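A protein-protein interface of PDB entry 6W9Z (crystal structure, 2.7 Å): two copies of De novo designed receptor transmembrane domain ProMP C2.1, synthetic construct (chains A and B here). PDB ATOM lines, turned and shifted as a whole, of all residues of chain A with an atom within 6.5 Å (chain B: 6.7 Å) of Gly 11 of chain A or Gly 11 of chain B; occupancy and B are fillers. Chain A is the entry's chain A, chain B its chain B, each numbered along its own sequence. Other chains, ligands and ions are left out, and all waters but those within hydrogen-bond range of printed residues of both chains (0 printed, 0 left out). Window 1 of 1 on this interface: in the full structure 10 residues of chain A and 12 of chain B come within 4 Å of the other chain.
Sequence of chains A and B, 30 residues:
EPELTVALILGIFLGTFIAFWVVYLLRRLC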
ATOM      1  N   VAL A   6      23.985  11.097   5.309  1.00  0.00           N
ATOM      2  CA  VAL A   6      23.472  11.275   3.954  1.00  0.00           C
ATOM      3  C   VAL A   6      22.273  10.365   3.707  1.00  0.00           C
ATOM      4  O   VAL A   6      21.375  10.708   2.928  1.00  0.00           O
ATOM      5  CB  VAL A   6      24.592  11.041   2.920  1.00  0.00           C
ATOM      6  CG1 VAL A   6      25.073   9.602   2.959  1.00  0.00           C
ATOM      7  CG2 VAL A   6      24.120  11.415   1.520  1.00  0.00           C
ATOM      8  N   ALA A   7      22.228   9.205   4.366  1.00  0.00           N
ATOM      9  CA  ALA A   7      21.059   8.342   4.249  1.00  0.00           C
ATOM     10  C   ALA A   7      19.842   8.988   4.895  1.00  0.00           C
ATOM     11  O   ALA A   7      18.723   8.879   4.380  1.00  0.00           O
ATOM     12  CB  ALA A   7      21.345   6.978   4.879  1.00  0.00           C
ATOM     13  N   LEU A   8      20.043   9.670   6.023  1.00  0.00           N
ATOM     14  CA  LEU A   8      18.936  10.352   6.686  1.00  0.00           C
ATOM     15  C   LEU A   8      18.479  11.566   5.889  1.00  0.00           C
ATOM     16  O   LEU A   8      17.274  11.803   5.743  1.00  0.00           O
ATOM     17  CB  LEU A   8      19.348  10.769   8.095  1.00  0.00           C
ATOM     18  CG  LEU A   8      18.222  11.286   8.994  1.00  0.00           C
ATOM     19  CD1 LEU A   8      17.455  10.127   9.617  1.00  0.00           C
ATOM     20  CD2 LEU A   8      18.773  12.210  10.062  1.00  0.00           C
ATOM     21  N   ILE A   9      19.427  12.349   5.368  1.00  0.00           N
ATOM     22  CA  ILE A   9      19.076  13.546   4.609  1.00  0.00           C
ATOM     23  C   ILE A   9      18.325  13.170   3.339  1.00  0.00           C
ATOM     24  O   ILE A   9      17.336  13.815   2.970  1.00  0.00           O
ATOM     25  CB  ILE A   9      20.337  14.373   4.301  1.00  0.00           C
ATOM     26  CG1 ILE A   9      20.933  14.941   5.590  1.00  0.00           C
ATOM     27  CG2 ILE A   9      20.017  15.495   3.328  1.00  0.00           C
ATOM     28  CD1 ILE A   9      20.014  15.898   6.316  1.00  0.00           C
ATOM     29  N   LEU A  10      18.778  12.117   2.652  1.00  0.00           N
ATOM     30  CA  LEU A  10      18.061  11.639   1.475  1.00  0.00           C
ATOM     31  C   LEU A  10      16.653  11.188   1.839  1.00  0.00           C
ATOM     32  O   LEU A  10      15.704  11.406   1.076  1.00  0.00           O
ATOM     33  CB  LEU A  10      18.835  10.499   0.813  1.00  0.00           C
ATOM     34  CG  LEU A  10      18.144   9.814  -0.370  1.00  0.00           C
ATOM     35  CD1 LEU A  10      17.889  10.809  -1.493  1.00  0.00           C
ATOM     36  CD2 LEU A  10      18.966   8.635  -0.870  1.00  0.00           C
ATOM     37  N   GLY A  11      16.495  10.558   3.004  1.00  0.00           N
ATOM     38  CA  GLY A  11      15.166  10.171   3.448  1.00  0.00           C
ATOM     39  C   GLY A  11      14.292  11.368   3.767  1.00  0.00           C
ATOM     40  O   GLY A  11      13.098  11.376   3.456  1.00  0.00           O
ATOM     41  N   ILE A  12      14.874  12.398   4.384  1.00  0.00           N
ATOM     42  CA  ILE A  12      14.112  13.601   4.709  1.00  0.00           C
ATOM     43  C   ILE A  12      13.641  14.296   3.438  1.00  0.00           C
ATOM     44  O   ILE A  12      12.498  14.766   3.358  1.00  0.00           O
ATOM     45  CB  ILE A  12      14.954  14.535   5.598  1.00  0.00           C
ATOM     46  CG1 ILE A  12      15.160  13.908   6.980  1.00  0.00           C
ATOM     47  CG2 ILE A  12      14.298  15.899   5.721  1.00  0.00           C
ATOM     48  CD1 ILE A  12      15.981  14.760   7.924  1.00  0.00           C
ATOM     49  N   PHE A  13      14.504  14.364   2.423  1.00  0.00           N
ATOM     50  CA  PHE A  13      14.103  14.947   1.147  1.00  0.00           C
ATOM     51  C   PHE A  13      13.033  14.101   0.470  1.00  0.00           C
ATOM     52  O   PHE A  13      12.038  14.629  -0.039  1.00  0.00           O
ATOM     53  CB  PHE A  13      15.319  15.100   0.233  1.00  0.00           C
ATOM     54  CG  PHE A  13      16.053  16.395   0.412  1.00  0.00           C
ATOM     55  CD1 PHE A  13      15.593  17.554  -0.191  1.00  0.00           C
ATOM     56  CD2 PHE A  13      17.207  16.453   1.174  1.00  0.00           C
ATOM     57  CE1 PHE A  13      16.266  18.748  -0.033  1.00  0.00           C
ATOM     58  CE2 PHE A  13      17.886  17.645   1.336  1.00  0.00           C
ATOM     59  CZ  PHE A  13      17.415  18.792   0.732  1.00  0.00           C
ATOM     60  N   LEU A  14      13.226  12.780   0.448  1.00  0.00           N
ATOM     61  CA  LEU A  14      12.234  11.900  -0.161  1.00  0.00           C
ATOM     62  C   LEU A  14      10.923  11.924   0.614  1.00  0.00           C
ATOM     63  O   LEU A  14       9.842  11.974   0.017  1.00  0.00           O
ATOM     64  CB  LEU A  14      12.779  10.476  -0.250  1.00  0.00           C
ATOM     65  CG  LEU A  14      13.735  10.197  -1.410  1.00  0.00           C
ATOM     66  CD1 LEU A  14      14.379   8.833  -1.248  1.00  0.00           C
ATOM     67  CD2 LEU A  14      12.996  10.289  -2.736  1.00  0.00           C
ATOM     68  N   GLY A  15      11.000  11.895   1.946  1.00  0.00           N
ATOM     69  CA  GLY A  15       9.785  11.928   2.746  1.00  0.00           C
ATOM     70  C   GLY A  15       8.989  13.204   2.551  1.00  0.00           C
ATOM     71  O   GLY A  15       7.757  13.178   2.513  1.00  0.00           O
ATOM     72  N   THR A  16       9.681  14.337   2.420  1.00  0.00           N
ATOM     73  CA  THR A  16       8.988  15.596   2.167  1.00  0.00           C
ATOM     74  C   THR A  16       8.352  15.603   0.783  1.00  0.00           C
ATOM     75  O   THR A  16       7.234  16.105   0.608  1.00  0.00           O
ATOM     76  CB  THR A  16       9.958  16.769   2.322  1.00  0.00           C
ATOM     77  OG1 THR A  16      10.509  16.764   3.646  1.00  0.00           O
ATOM     78  CG2 THR A  16       9.242  18.092   2.088  1.00  0.00           C
ATOM     79  N   VAL B   6      17.486   1.755   7.862  1.00  0.00           N
ATOM     80  CA  VAL B   6      16.722   2.321   8.971  1.00  0.00           C
ATOM     81  C   VAL B   6      16.850   3.838   8.983  1.00  0.00           C
ATOM     82  O   VAL B   6      15.858   4.561   9.128  1.00  0.00           O
ATOM     83  CB  VAL B   6      17.180   1.707  10.305  1.00  0.00           C
ATOM     84  CG1 VAL B   6      16.497   2.404  11.470  1.00  0.00           C
ATOM     85  CG2 VAL B   6      16.890   0.217  10.329  1.00  0.00           C
ATOM     86  N   ALA B   7      18.078   4.342   8.828  1.00  0.00           N
ATOM     87  CA  ALA B   7      18.283   5.786   8.768  1.00  0.00           C
ATOM     88  C   ALA B   7      17.538   6.407   7.594  1.00  0.00           C
ATOM     89  O   ALA B   7      17.076   7.551   7.685  1.00  0.00           O
ATOM     90  CB  ALA B   7      19.775   6.105   8.678  1.00  0.00           C
ATOM     91  N   LEU B   8      17.409   5.672   6.489  1.00  0.00           N
ATOM     92  CA  LEU B   8      16.646   6.165   5.348  1.00  0.00           C
ATOM     93  C   LEU B   8      15.157   6.222   5.672  1.00  0.00           C
ATOM     94  O   LEU B   8      14.497   7.240   5.430  1.00  0.00           O
ATOM     95  CB  LEU B   8      16.901   5.279   4.130  1.00  0.00           C
ATOM     96  CG  LEU B   8      16.263   5.712   2.809  1.00  0.00           C
ATOM     97  CD1 LEU B   8      16.833   7.047   2.353  1.00  0.00           C
ATOM     98  CD2 LEU B   8      16.470   4.646   1.745  1.00  0.00           C
ATOM     99  N   ILE B   9      14.614   5.134   6.221  1.00  0.00           N
ATOM    100  CA  ILE B   9      13.191   5.092   6.551  1.00  0.00           C
ATOM    101  C   ILE B   9      12.868   6.088   7.658  1.00  0.00           C
ATOM    102  O   ILE B   9      11.811   6.730   7.645  1.00  0.00           O
ATOM    103  CB  ILE B   9      12.778   3.657   6.931  1.00  0.00           C
ATOM    104  CG1 ILE B   9      12.958   2.718   5.735  1.00  0.00           C
ATOM    105  CG2 ILE B   9      11.342   3.621   7.433  1.00  0.00           C
ATOM    106  CD1 ILE B   9      12.579   1.284   6.024  1.00  0.00           C
ATOM    107  N   LEU B  10      13.772   6.235   8.631  1.00  0.00           N
ATOM    108  CA  LEU B  10      13.585   7.240   9.672  1.00  0.00           C
ATOM    109  C   LEU B  10      13.486   8.636   9.072  1.00  0.00           C
ATOM    110  O   LEU B  10      12.641   9.441   9.480  1.00  0.00           O
ATOM    111  CB  LEU B  10      14.728   7.168  10.685  1.00  0.00           C
ATOM    112  CG  LEU B  10      14.395   6.580  12.057  1.00  0.00           C
ATOM    113  CD1 LEU B  10      13.792   5.192  11.917  1.00  0.00           C
ATOM    114  CD2 LEU B  10      15.641   6.543  12.931  1.00  0.00           C
ATOM    115  N   GLY B  11      14.342   8.943   8.097  1.00  0.00           N
ATOM    116  CA  GLY B  11      14.276  10.243   7.455  1.00  0.00           C
ATOM    117  C   GLY B  11      13.006  10.433   6.647  1.00  0.00           C
ATOM    118  O   GLY B  11      12.466  11.536   6.580  1.00  0.00           O
ATOM    119  N   ILE B  12      12.510   9.354   6.038  1.00  0.00           N
ATOM    120  CA  ILE B  12      11.294   9.443   5.232  1.00  0.00           C
ATOM    121  C   ILE B  12      10.107   9.834   6.101  1.00  0.00           C
ATOM    122  O   ILE B  12       9.366  10.773   5.786  1.00  0.00           O
ATOM    123  CB  ILE B  12      11.043   8.115   4.495  1.00  0.00           C
ATOM    124  CG1 ILE B  12      12.013   7.960   3.322  1.00  0.00           C
ATOM    125  CG2 ILE B  12       9.595   8.030   4.024  1.00  0.00           C
ATOM    126  CD1 ILE B  12      11.811   6.691   2.524  1.00  0.00           C
ATOM    127  N   PHE B  13       9.906   9.117   7.210  1.00  0.00           N
ATOM    128  CA  PHE B  13       8.816   9.459   8.118  1.00  0.00           C
ATOM    129  C   PHE B  13       9.041  10.822   8.759  1.00  0.00           C
ATOM    130  O   PHE B  13       8.085  11.568   9.000  1.00  0.00           O
ATOM    131  CB  PHE B  13       8.661   8.376   9.186  1.00  0.00           C
ATOM    132  CG  PHE B  13       7.824   7.212   8.750  1.00  0.00           C
ATOM    133  CD1 PHE B  13       6.443   7.270   8.829  1.00  0.00           C
ATOM    134  CD2 PHE B  13       8.415   6.060   8.260  1.00  0.00           C
ATOM    135  CE1 PHE B  13       5.667   6.204   8.429  1.00  0.00           C
ATOM    136  CE2 PHE B  13       7.643   4.988   7.858  1.00  0.00           C
ATOM    137  CZ  PHE B  13       6.268   5.062   7.944  1.00  0.00           C
ATOM    138  N   LEU B  14      10.300  11.166   9.043  1.00  0.00           N
ATOM    139  CA  LEU B  14      10.612  12.512   9.507  1.00  0.00           C
ATOM    140  C   LEU B  14      10.302  13.545   8.431  1.00  0.00           C
ATOM    141  O   LEU B  14       9.888  14.667   8.738  1.00  0.00           O
ATOM    142  CB  LEU B  14      12.078  12.594   9.933  1.00  0.00           C
ATOM    143  CG  LEU B  14      12.564  13.929  10.500  1.00  0.00           C
ATOM    144  CD1 LEU B  14      11.699  14.356  11.672  1.00  0.00           C
ATOM    145  CD2 LEU B  14      14.022  13.822  10.919  1.00  0.00           C
ATOM    146  N   GLY B  15      10.487  13.177   7.162  1.00  0.00           N
ATOM    147  CA  GLY B  15      10.188  14.102   6.081  1.00  0.00           C
ATOM    148  C   GLY B  15       8.706  14.391   5.938  1.00  0.00           C
ATOM    149  O   GLY B  15       8.316  15.505   5.586  1.00  0.00           O
ATOM    150  N   THR B  16       7.860  13.391   6.210  1.00  0.00           N
ATOM    151  CA  THR B  16       6.418  13.604   6.134  1.00  0.00           C
ATOM    152  C   THR B  16       5.943  14.606   7.179  1.00  0.00           C
ATOM    153  O   THR B  16       4.991  15.353   6.929  1.00  0.00           O
ATOM    154  CB  THR B  16       5.679  12.276   6.293  1.00  0.00           C
ATOM    155  OG1 THR B  16       5.924  11.742   7.600  1.00  0.00           O
ATOM    156  CG2 THR B  16       6.156  11.275   5.252  1.00  0.00           C
ATOM    157  N   ILE B  18       7.957  17.098   8.295  1.00  0.00           N
ATOM    158  CA  ILE B  18       8.525  18.374   7.872  1.00  0.00           C
ATOM    159  C   ILE B  18       7.687  19.003   6.767  1.00  0.00           C
ATOM    160  O   ILE B  18       7.586  20.233   6.678  1.00  0.00           O
ATOM    161  CB  ILE B  18       9.992  18.175   7.441  1.00  0.00           C
ATOM    162  CG1 ILE B  18      10.837  17.726   8.634  1.00  0.00           C
ATOM    163  CG2 ILE B  18      10.562  19.448   6.837  1.00  0.00           C
ATOM    164  CD1 ILE B  18      12.302  17.546   8.313  1.00  0.00           C
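The backbone carbonyl oxygen (O) of Gly 11 of chain B sits close to the backbone carbonyl oxygen (O) of Gly 11 of chain A, at 3.2 Å.
The backbone NH (N) of Ile 12 of chain B sits close to the backbone carbonyl oxygen (O) of Gly 11 of chain A (3.3 Å).
The side-chain hydroxyl (OG1) of Thr 16 of chain A is in hydrogen-bond range of the backbone carbonyl oxygen (O) of Gly 15 of chain B.
The backbone NH (N) of Ile 12 of chain A lies close to the backbone carbonyl oxygen (O) of Gly 11 of chain B (3.4 Å).
Of the 12 printed residues of chain B, 8 touch a printed residue of chain A.
Hydrophobic or aromatic side chains of chain B that line the printed part of chain A: Leu 8, Ile 12, Leu 14 and Ile 18.
Hydrophobic or aromatic side chains of chain A that line the printed part of chain B: Leu 8 and Ile 12.
Among the printed residues, 15 pairs touch across the chains.
Among the printed residues, no Asp or Glu carboxylate lies within 4 Å of a Lys or Arg side-chain nitrogen of the other chain.
O of Phe 13 of chain B sits at hydrogen-bond distance from OG1 of Thr 16 of chain B.
The backbone carbonyl oxygen (O) of Ile 12 of chain A lies within hydrogen-bond range of the side-chain hydroxyl (OG1) of Thr 16 of chain A.
Gly 11 of chain A touches three residues of chain B.
Of the printed residues of chain B, Gly 15 of chain A touches Ile 12 (3.3 Å), Gly 15 (3.6 Å) and Thr 16 (3.7 Å).
Printed residues of chain A within 4 Å of Ala 7 of chain B: Ala 7 (3.9 Å) and Leu 8 (3.2 Å).
Of the printed residues of chain A, Leu 8 of chain B touches Ala 7 and Gly 11.
Gly 11 of chain B touches three residues of chain A.
Of the printed residues of chain A, Ile 12 of chain B touches Gly 11 (3.2 Å) and Gly 15 (3.3 Å).
The nearest residue of chain B that does not touch Gly 11 of chain A is Gly 15 of chain B (4.8 Å).
The nearest residue of chain A that does not touch Gly 11 of chain B is Gly 15 of chain A (4.7 Å).
The nearest printed residue of chain B that does not touch Thr 16 of chain A is Ile 18 of chain B (4.1 Å).
Among the printed residues, pairs that only touch across the chains: Ala 7 of chain A with Ala 7 of chain B (3.9 Å), Ala 7 of chain A with Leu 8 of chain B (3.3 Å), Leu 8 of chain A with Ala 7 of chain B (3.2 Å), Leu 8 of chain A with Gly 11 of chain B (3.7 Å), Gly 11 of chain A with Leu 8 of chain B (3.6 Å), Ile 12 of chain A with Leu 14 of chain B (3.7 Å), Ile 12 of chain A with Gly 15 of chain B (3.6 Å), Ile 12 of chain A with Ile 18 of chain B (3.7 Å), Gly 15 of chain A with Ile 12 of chain B (3.3 Å), Gly 15 of chain A with Gly 15 of chain B (3.6 Å) and Gly 15 of chain A with Thr 16 of chain B (3.7 Å).
Ala 7 of chain A touches its own counterpart, Ala 7 of chain B.
Gly 11 of chain B touches its own counterpart, Gly 11 of chain A.
Gly 11 of chain A touches Ile 12 of chain B, and with the chains exchanged Ile 12 of chain A touches Gly 11 of chain B.
Gly 15 of chain B touches its own counterpart, Gly 15 of chain A.
Positions printed for both chains: 6, 7, 8, 9, 10, 11, 12, 13, 14, 15 and 16.
Of the 15 pairs that touch across the chains among the printed residues, 13 have their exchanged pair printed and touching as well.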
